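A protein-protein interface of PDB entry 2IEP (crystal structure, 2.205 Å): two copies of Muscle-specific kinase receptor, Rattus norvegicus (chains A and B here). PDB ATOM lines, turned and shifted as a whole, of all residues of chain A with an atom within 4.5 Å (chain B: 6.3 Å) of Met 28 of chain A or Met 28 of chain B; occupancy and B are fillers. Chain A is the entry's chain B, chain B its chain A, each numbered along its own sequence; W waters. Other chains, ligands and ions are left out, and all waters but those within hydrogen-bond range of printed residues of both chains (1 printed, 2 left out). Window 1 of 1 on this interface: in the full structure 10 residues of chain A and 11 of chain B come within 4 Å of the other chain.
Water W1 lies within hydrogen-bond range of the side-chain carboxylate (OE2) of Glu 59 of chain A (2.7 Å), the backbone NH (N) of Glu 15 of chain B (3.3 Å) and the backbone NH (N) of Met 28 of chain B (3.4 Å).
Of the printed residues of chain B, Thr 12 of chain A touches Ala 30. Of chain B, only Met 28, Glu 59 and Gln 62 come within 4 Å of Met 28 of chain A. Cys 29 of chain A touches none of the printed residues of chain B. Of the printed residues of chain B, Glu 59 of chain A touches Glu 15 and Met 28. Printed residues of chain B within 4 Å of Gln 62 of chain A: Met 28 (3.8 Å). Met 28 of chain B touches four residues of chain A. Printed residues of chain A within 4 Å of Ala 30 of chain B: Thr 12 (3.8 Å). Of the printed residues of chain A, Glu 59 of chain B touches Met 28. The nearest residue of chain A that does not touch Met 28 of chain B is Ala 30 of chain A (4.4 Å).
The side-chain carboxylate (OE2) of Glu 15 of chain B sits close to the side-chain carboxylate (OE1) of Glu 59 of chain A, at 3.1 Å.
Among the printed residues, merely in contact across the chains: Thr 12 of chain A with Ala 30 of chain B, Met 28 of chain A with Met 28 of chain B, Met 28 of chain A with Glu 59 of chain B, Met 28 of chain A with Gln 62 of chain B, Ala 30 of chain A with Thr 12 of chain B, Glu 59 of chain A with Met 28 of chain B, Gln 62 of chain A with Met 28 of chain B, Leu 63 of chain A with Thr 26 of chain B, Leu 63 of chain A with Met 28 of chain B and Leu 63 of chain A with Leu 63 of chain B.
The backbone carbonyl oxygen (O) of Glu 59 of chain B is in hydrogen-bond range of the side-chain amide nitrogen (NE2) of Gln 62 of chain B, at 2.9 Å. The backbone NH (N) of Cys 29 of chain A is in hydrogen-bond range of the backbone carbonyl oxygen (O) of Gln 62 of chain A, 2.7 Å away. OG1 of Thr 12 of chain A is in hydrogen-bond range of O of Met 28 of chain A, at 3.0 Å. O of Glu 59 of chain A lies within hydrogen-bond range of NE2 of Gln 62 of chain A, at 3.1 Å. The side-chain hydroxyl (OG1) of Thr 12 of chain B lies within hydrogen-bond range of the backbone NH (N) of Ala 30 of chain B (3.1 Å). SG of Cys 29 of chain B is disulfide-bonded to SG of Cys 79 of chain B.
Thr 12 of chain A touches Ala 30 of chain B, and with the chains exchanged Ala 30 of chain A touches Thr 12 of chain B. Met 28 of chain A touches Gln 62 of chain B, and with the chains exchanged Gln 62 of chain A touches Met 28 of chain B. Leu 63 of chain A touches Thr 26 of chain B, but with the chains exchanged Thr 26 of chain A does not touch Leu 63 of chain B (4.05 Å). Leu 63 of chain A touches Met 28 of chain B, but with the chains exchanged Met 28 of chain A does not touch Leu 63 of chain B (4.05 Å). 10 positions are printed for both chains. Of the 11 pairs that touch across the chains among the printed residues, 8 have their exchanged pair printed and touching as well.
Of the 10 printed residues of chain A, 6 touch a printed residue of chain B. Hydrophobic or aromatic side chains of chain A within 4 Å of the printed part of chain B: Met 28, Ala 30 and Leu 63. Among the printed residues, no Asp or Glu carboxylate lies within 4 Å of a Lys or Arg side-chain nitrogen of the other chain.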
ATOM      1  N   THR A  12      -3.253  23.588  -9.614  1.00  0.00           N
ATOM      2  CA  THR A  12      -4.671  23.883  -9.803  1.00  0.00           C
ATOM      3  C   THR A  12      -5.381  23.920  -8.458  1.00  0.00           C
ATOM      4  O   THR A  12      -5.897  22.904  -7.990  1.00  0.00           O
ATOM      5  CB  THR A  12      -5.372  22.865 -10.734  1.00  0.00           C
ATOM      6  OG1 THR A  12      -5.205  21.552 -10.198  1.00  0.00           O
ATOM      7  CG2 THR A  12      -4.782  22.916 -12.131  1.00  0.00           C
ATOM      8  N   LEU A  14      -8.110  24.014  -5.750  1.00  0.00           N
ATOM      9  CA  LEU A  14      -9.481  23.524  -5.815  1.00  0.00           C
ATOM     10  C   LEU A  14     -10.442  24.716  -5.806  1.00  0.00           C
ATOM     11  O   LEU A  14     -10.162  25.760  -5.194  1.00  0.00           O
ATOM     12  CB  LEU A  14      -9.812  22.544  -4.672  1.00  0.00           C
ATOM     13  CG  LEU A  14      -9.043  21.228  -4.471  1.00  0.00           C
ATOM     14  CD1 LEU A  14      -9.807  20.356  -3.499  1.00  0.00           C
ATOM     15  CD2 LEU A  14      -8.780  20.468  -5.762  1.00  0.00           C
ATOM     16  N   THR A  26     -16.173  16.393 -10.381  1.00  0.00           N
ATOM     17  CA  THR A  26     -14.754  16.105 -10.313  1.00  0.00           C
ATOM     18  C   THR A  26     -13.978  17.270  -9.675  1.00  0.00           C
ATOM     19  O   THR A  26     -14.229  18.423  -9.965  1.00  0.00           O
ATOM     20  CB  THR A  26     -14.174  15.770 -11.733  1.00  0.00           C
ATOM     21  OG1 THR A  26     -14.731  14.531 -12.199  1.00  0.00           O
ATOM     22  CG2 THR A  26     -12.658  15.616 -11.688  1.00  0.00           C
ATOM     23  N   PHE A  27     -13.034  16.931  -8.802  1.00  0.00           N
ATOM     24  CA  PHE A  27     -12.043  17.877  -8.291  1.00  0.00           C
ATOM     25  C   PHE A  27     -10.694  17.614  -8.937  1.00  0.00           C
ATOM     26  O   PHE A  27     -10.237  16.485  -8.990  1.00  0.00           O
ATOM     27  CB  PHE A  27     -11.941  17.762  -6.757  1.00  0.00           C
ATOM     28  CG  PHE A  27     -13.068  18.419  -6.039  1.00  0.00           C
ATOM     29  CD1 PHE A  27     -13.080  19.802  -5.854  1.00  0.00           C
ATOM     30  CD2 PHE A  27     -14.141  17.674  -5.576  1.00  0.00           C
ATOM     31  CE1 PHE A  27     -14.124  20.423  -5.199  1.00  0.00           C
ATOM     32  CE2 PHE A  27     -15.191  18.293  -4.932  1.00  0.00           C
ATOM     33  CZ  PHE A  27     -15.179  19.679  -4.743  1.00  0.00           C
ATOM     34  N   MET A  28     -10.058  18.684  -9.406  1.00  0.00           N
ATOM     35  CA  MET A  28      -8.751  18.625 -10.042  1.00  0.00           C
ATOM     36  C   MET A  28      -7.653  19.212  -9.117  1.00  0.00           C
ATOM     37  O   MET A  28      -7.655  20.409  -8.806  1.00  0.00           O
ATOM     38  CB  MET A  28      -8.815  19.398 -11.370  1.00  0.00           C
ATOM     39  CG  MET A  28      -7.472  19.636 -12.034  1.00  0.00           C
ATOM     40  SD  MET A  28      -7.586  20.311 -13.712  1.00  0.00           S
ATOM     41  CE  MET A  28      -8.217  21.953 -13.447  1.00  0.00           C
ATOM     42  N   CYS A  29      -6.718  18.359  -8.717  1.00  0.00           N
ATOM     43  CA  CYS A  29      -5.615  18.719  -7.816  1.00  0.00           C
ATOM     44  C   CYS A  29      -4.317  18.324  -8.477  1.00  0.00           C
ATOM     45  O   CYS A  29      -3.661  17.375  -8.053  1.00  0.00           O
ATOM     46  CB  CYS A  29      -5.760  17.980  -6.478  1.00  0.00           C
ATOM     47  SG  CYS A  29      -4.534  18.396  -5.202  1.00  0.00           S
ATOM     48  N   ALA A  30      -3.969  19.046  -9.536  1.00  0.00           N
ATOM     49  CA  ALA A  30      -2.745  18.803 -10.290  1.00  0.00           C
ATOM     50  C   ALA A  30      -1.551  19.218  -9.443  1.00  0.00           C
ATOM     51  O   ALA A  30      -1.561  20.281  -8.835  1.00  0.00           O
ATOM     52  CB  ALA A  30      -2.773  19.577 -11.600  1.00  0.00           C
ATOM     53  N   GLU A  59      -5.565   9.378 -12.025  1.00  0.00           N
ATOM     54  CA  GLU A  59      -4.292  10.060 -12.319  1.00  0.00           C
ATOM     55  C   GLU A  59      -3.442  10.335 -11.083  1.00  0.00           C
ATOM     56  O   GLU A  59      -3.083  11.482 -10.801  1.00  0.00           O
ATOM     57  CB  GLU A  59      -4.518  11.344 -13.136  1.00  0.00           C
ATOM     58  CG  GLU A  59      -4.901  11.068 -14.591  1.00  0.00           C
ATOM     59  CD  GLU A  59      -4.816  12.296 -15.485  1.00  0.00           C
ATOM     60  OE1 GLU A  59      -3.841  13.079 -15.363  1.00  0.00           O
ATOM     61  OE2 GLU A  59      -5.715  12.454 -16.347  1.00  0.00           O
ATOM     62  N   GLN A  62      -4.690  12.926  -8.448  1.00  0.00           N
ATOM     63  CA  GLN A  62      -4.922  14.289  -8.913  1.00  0.00           C
ATOM     64  C   GLN A  62      -6.369  14.568  -9.284  1.00  0.00           C
ATOM     65  O   GLN A  62      -6.779  15.726  -9.332  1.00  0.00           O
ATOM     66  CB  GLN A  62      -4.013  14.626 -10.090  1.00  0.00           C
ATOM     67  CG  GLN A  62      -2.539  14.653  -9.740  1.00  0.00           C
ATOM     68  CD  GLN A  62      -1.666  14.921 -10.943  1.00  0.00           C
ATOM     69  OE1 GLN A  62      -1.008  15.953 -11.019  1.00  0.00           O
ATOM     70  NE2 GLN A  62      -1.659  13.992 -11.894  1.00  0.00           N
ATOM     71  N   LEU A  63      -7.129  13.510  -9.548  1.00  0.00           N
ATOM     72  CA  LEU A  63      -8.557  13.617  -9.857  1.00  0.00           C
ATOM     73  C   LEU A  63      -9.388  12.843  -8.870  1.00  0.00           C
ATOM     74  O   LEU A  63      -9.198  11.641  -8.700  1.00  0.00           O
ATOM     75  CB  LEU A  63      -8.881  13.114 -11.277  1.00  0.00           C
ATOM     76  CG  LEU A  63      -8.321  13.943 -12.432  1.00  0.00           C
ATOM     77  CD1 LEU A  63      -8.544  13.247 -13.765  1.00  0.00           C
ATOM     78  CD2 LEU A  63      -8.895  15.371 -12.437  1.00  0.00           C
ATOM     79  N   ILE B  10       0.713  23.493 -21.163  1.00  0.00           N
ATOM     80  CA  ILE B  10      -0.046  22.371 -20.600  1.00  0.00           C
ATOM     81  C   ILE B  10       0.808  21.657 -19.548  1.00  0.00           C
ATOM     82  O   ILE B  10       1.805  20.998 -19.875  1.00  0.00           O
ATOM     83  CB  ILE B  10      -0.553  21.400 -21.696  1.00  0.00           C
ATOM     84  CG1 ILE B  10      -1.546  22.134 -22.620  1.00  0.00           C
ATOM     85  CG2 ILE B  10      -1.152  20.104 -21.058  1.00  0.00           C
ATOM     86  CD1 ILE B  10      -1.829  21.430 -23.953  1.00  0.00           C
ATOM     87  N   THR B  12      -0.229  19.310 -17.363  1.00  0.00           N
ATOM     88  CA  THR B  12      -0.527  17.894 -17.225  1.00  0.00           C
ATOM     89  C   THR B  12      -0.755  17.279 -18.592  1.00  0.00           C
ATOM     90  O   THR B  12      -1.871  17.313 -19.098  1.00  0.00           O
ATOM     91  CB  THR B  12      -1.762  17.635 -16.330  1.00  0.00           C
ATOM     92  OG1 THR B  12      -2.933  18.160 -16.970  1.00  0.00           O
ATOM     93  CG2 THR B  12      -1.589  18.256 -14.952  1.00  0.00           C
ATOM     94  N   PRO B  13       0.296  16.696 -19.188  1.00  0.00           N
ATOM     95  CA  PRO B  13       0.129  16.057 -20.473  1.00  0.00           C
ATOM     96  C   PRO B  13      -0.944  14.974 -20.379  1.00  0.00           C
ATOM     97  O   PRO B  13      -1.089  14.332 -19.333  1.00  0.00           O
ATOM     98  CB  PRO B  13       1.500  15.417 -20.731  1.00  0.00           C
ATOM     99  CG  PRO B  13       2.451  16.208 -19.903  1.00  0.00           C
ATOM    100  CD  PRO B  13       1.680  16.584 -18.688  1.00  0.00           C
ATOM    101  N   LEU B  14      -1.690  14.787 -21.461  1.00  0.00           N
ATOM    102  CA  LEU B  14      -2.717  13.758 -21.515  1.00  0.00           C
ATOM    103  C   LEU B  14      -2.091  12.383 -21.405  1.00  0.00           C
ATOM    104  O   LEU B  14      -1.000  12.135 -21.944  1.00  0.00           O
ATOM    105  CB  LEU B  14      -3.516  13.865 -22.814  1.00  0.00           C
ATOM    106  CG  LEU B  14      -4.872  14.566 -22.767  1.00  0.00           C
ATOM    107  CD1 LEU B  14      -4.904  15.807 -21.872  1.00  0.00           C
ATOM    108  CD2 LEU B  14      -5.385  14.873 -24.162  1.00  0.00           C
ATOM    109  N   GLU B  15      -2.795  11.489 -20.719  1.00  0.00           N
ATOM    110  CA  GLU B  15      -2.332  10.124 -20.513  1.00  0.00           C
ATOM    111  C   GLU B  15      -3.160   9.150 -21.348  1.00  0.00           C
ATOM    112  O   GLU B  15      -4.025   9.564 -22.107  1.00  0.00           O
ATOM    113  CB  GLU B  15      -2.407   9.790 -19.019  1.00  0.00           C
ATOM    114  CG  GLU B  15      -1.533  10.679 -18.149  1.00  0.00           C
ATOM    115  CD  GLU B  15      -1.623  10.342 -16.661  1.00  0.00           C
ATOM    116  OE1 GLU B  15      -1.915   9.172 -16.322  1.00  0.00           O
ATOM    117  OE2 GLU B  15      -1.383  11.250 -15.824  1.00  0.00           O
ATOM    118  N   THR B  26     -12.254  10.491 -17.730  1.00  0.00           N
ATOM    119  CA  THR B  26     -11.891  11.914 -17.671  1.00  0.00           C
ATOM    120  C   THR B  26     -10.471  12.145 -18.172  1.00  0.00           C
ATOM    121  O   THR B  26      -9.531  11.438 -17.761  1.00  0.00           O
ATOM    122  CB  THR B  26     -12.012  12.472 -16.219  1.00  0.00           C
ATOM    123  OG1 THR B  26     -13.372  12.421 -15.813  1.00  0.00           O
ATOM    124  CG2 THR B  26     -11.567  13.921 -16.114  1.00  0.00           C
ATOM    125  N   PHE B  27     -10.332  13.130 -19.063  1.00  0.00           N
ATOM    126  CA  PHE B  27      -9.023  13.660 -19.464  1.00  0.00           C
ATOM    127  C   PHE B  27      -8.738  14.973 -18.766  1.00  0.00           C
ATOM    128  O   PHE B  27      -9.615  15.851 -18.671  1.00  0.00           O
ATOM    129  CB  PHE B  27      -8.925  13.844 -20.985  1.00  0.00           C
ATOM    130  CG  PHE B  27      -8.802  12.552 -21.749  1.00  0.00           C
ATOM    131  CD1 PHE B  27      -7.556  11.943 -21.919  1.00  0.00           C
ATOM    132  CD2 PHE B  27      -9.927  11.943 -22.300  1.00  0.00           C
ATOM    133  CE1 PHE B  27      -7.423  10.741 -22.619  1.00  0.00           C
ATOM    134  CE2 PHE B  27      -9.820  10.740 -23.000  1.00  0.00           C
ATOM    135  CZ  PHE B  27      -8.558  10.136 -23.166  1.00  0.00           C
ATOM    136  N   MET B  28      -7.509  15.111 -18.274  1.00  0.00           N
ATOM    137  CA  MET B  28      -7.127  16.332 -17.581  1.00  0.00           C
ATOM    138  C   MET B  28      -6.085  17.124 -18.372  1.00  0.00           C
ATOM    139  O   MET B  28      -4.980  16.649 -18.598  1.00  0.00           O
ATOM    140  CB  MET B  28      -6.636  16.029 -16.166  1.00  0.00           C
ATOM    141  CG  MET B  28      -5.892  17.192 -15.531  1.00  0.00           C
ATOM    142  SD  MET B  28      -5.549  16.981 -13.776  1.00  0.00           S
ATOM    143  CE  MET B  28      -4.568  15.486 -13.780  1.00  0.00           C
ATOM    144  N   CYS B  29      -6.461  18.331 -18.783  1.00  0.00           N
ATOM    145  CA  CYS B  29      -5.599  19.193 -19.594  1.00  0.00           C
ATOM    146  C   CYS B  29      -5.421  20.531 -18.895  1.00  0.00           C
ATOM    147  O   CYS B  29      -5.926  21.560 -19.372  1.00  0.00           O
ATOM    148  CB  CYS B  29      -6.224  19.417 -20.978  1.00  0.00           C
ATOM    149  SG  CYS B  29      -5.257  20.454 -22.115  1.00  0.00           S
ATOM    150  N   ALA B  30      -4.738  20.513 -17.751  1.00  0.00           N
ATOM    151  CA  ALA B  30      -4.569  21.720 -16.954  1.00  0.00           C
ATOM    152  C   ALA B  30      -3.582  22.673 -17.647  1.00  0.00           C
ATOM    153  O   ALA B  30      -2.547  22.234 -18.168  1.00  0.00           O
ATOM    154  CB  ALA B  30      -4.116  21.367 -15.549  1.00  0.00           C
ATOM    155  N   TRP B  41     -10.882  20.574 -28.028  1.00  0.00           N
ATOM    156  CA  TRP B  41     -10.612  19.143 -27.951  1.00  0.00           C
ATOM    157  C   TRP B  41     -11.012  18.479 -29.245  1.00  0.00           C
ATOM    158  O   TRP B  41     -12.011  18.863 -29.841  1.00  0.00           O
ATOM    159  CB  TRP B  41     -11.425  18.494 -26.823  1.00  0.00           C
ATOM    160  CG  TRP B  41     -11.034  18.902 -25.432  1.00  0.00           C
ATOM    161  CD1 TRP B  41     -11.385  20.061 -24.770  1.00  0.00           C
ATOM    162  CD2 TRP B  41     -10.233  18.140 -24.516  1.00  0.00           C
ATOM    163  NE1 TRP B  41     -10.833  20.059 -23.492  1.00  0.00           N
ATOM    164  CE2 TRP B  41     -10.137  18.890 -23.311  1.00  0.00           C
ATOM    165  CE3 TRP B  41      -9.598  16.887 -24.591  1.00  0.00           C
ATOM    166  CZ2 TRP B  41      -9.428  18.430 -22.200  1.00  0.00           C
ATOM    167  CZ3 TRP B  41      -8.888  16.432 -23.470  1.00  0.00           C
ATOM    168  CH2 TRP B  41      -8.812  17.208 -22.300  1.00  0.00           C
ATOM    169  N   GLU B  59     -13.996  23.351 -15.523  1.00  0.00           N
ATOM    170  CA  GLU B  59     -12.774  24.116 -15.268  1.00  0.00           C
ATOM    171  C   GLU B  59     -12.182  24.717 -16.563  1.00  0.00           C
ATOM    172  O   GLU B  59     -11.003  24.540 -16.903  1.00  0.00           O
ATOM    173  CB  GLU B  59     -11.783  23.292 -14.429  1.00  0.00           C
ATOM    174  CG  GLU B  59     -12.343  23.026 -13.017  1.00  0.00           C
ATOM    175  CD  GLU B  59     -11.282  22.697 -11.950  1.00  0.00           C
ATOM    176  OE1 GLU B  59     -10.247  23.422 -11.797  1.00  0.00           O
ATOM    177  OE2 GLU B  59     -11.516  21.703 -11.224  1.00  0.00           O
ATOM    178  N   GLN B  62     -10.392  22.531 -19.194  1.00  0.00           N
ATOM    179  CA  GLN B  62      -9.265  21.750 -18.684  1.00  0.00           C
ATOM    180  C   GLN B  62      -9.670  20.325 -18.293  1.00  0.00           C
ATOM    181  O   GLN B  62      -8.838  19.407 -18.287  1.00  0.00           O
ATOM    182  CB  GLN B  62      -8.655  22.432 -17.468  1.00  0.00           C
ATOM    183  CG  GLN B  62      -8.025  23.781 -17.747  1.00  0.00           C
ATOM    184  CD  GLN B  62      -7.537  24.443 -16.483  1.00  0.00           C
ATOM    185  OE1 GLN B  62      -6.343  24.473 -16.227  1.00  0.00           O
ATOM    186  NE2 GLN B  62      -8.461  24.981 -15.684  1.00  0.00           N
ATOM    187  N   LEU B  63     -10.945  20.155 -17.949  1.00  0.00           N
ATOM    188  CA  LEU B  63     -11.482  18.833 -17.694  1.00  0.00           C
ATOM    189  C   LEU B  63     -12.503  18.441 -18.746  1.00  0.00           C
ATOM    190  O   LEU B  63     -13.497  19.133 -18.946  1.00  0.00           O
ATOM    191  CB  LEU B  63     -12.137  18.766 -16.310  1.00  0.00           C
ATOM    192  CG  LEU B  63     -11.246  18.875 -15.065  1.00  0.00           C
ATOM    193  CD1 LEU B  63     -12.144  19.003 -13.840  1.00  0.00           C
ATOM    194  CD2 LEU B  63     -10.369  17.653 -14.969  1.00  0.00           C
ATOM    195  N   LEU B  64     -12.252  17.316 -19.401  1.00  0.00           N
ATOM    196  CA  LEU B  64     -13.236  16.693 -20.275  1.00  0.00           C
ATOM    197  C   LEU B  64     -13.608  15.300 -19.752  1.00  0.00           C
ATOM    198  O   LEU B  64     -12.764  14.420 -19.676  1.00  0.00           O
ATOM    199  CB  LEU B  64     -12.706  16.615 -21.711  1.00  0.00           C
ATOM    200  CG  LEU B  64     -13.623  15.953 -22.751  1.00  0.00           C
ATOM    201  CD1 LEU B  64     -13.432  16.649 -24.114  1.00  0.00           C
ATOM    202  CD2 LEU B  64     -13.384  14.436 -22.867  1.00  0.00           C
ATOM    203  N   CYS B  79      -5.992  17.982 -26.590  1.00  0.00           N
ATOM    204  CA  CYS B  79      -6.423  19.292 -26.150  1.00  0.00           C
ATOM    205  C   CYS B  79      -5.441  20.345 -26.686  1.00  0.00           C
ATOM    206  O   CYS B  79      -4.230  20.100 -26.763  1.00  0.00           O
ATOM    207  CB  CYS B  79      -6.554  19.367 -24.622  1.00  0.00           C
ATOM    208  SG  CYS B  79      -4.996  19.183 -23.681  1.00  0.00           S
HETATM  209  O   HOH W   1      -5.338  12.631 -19.028  1.00  0.00           O
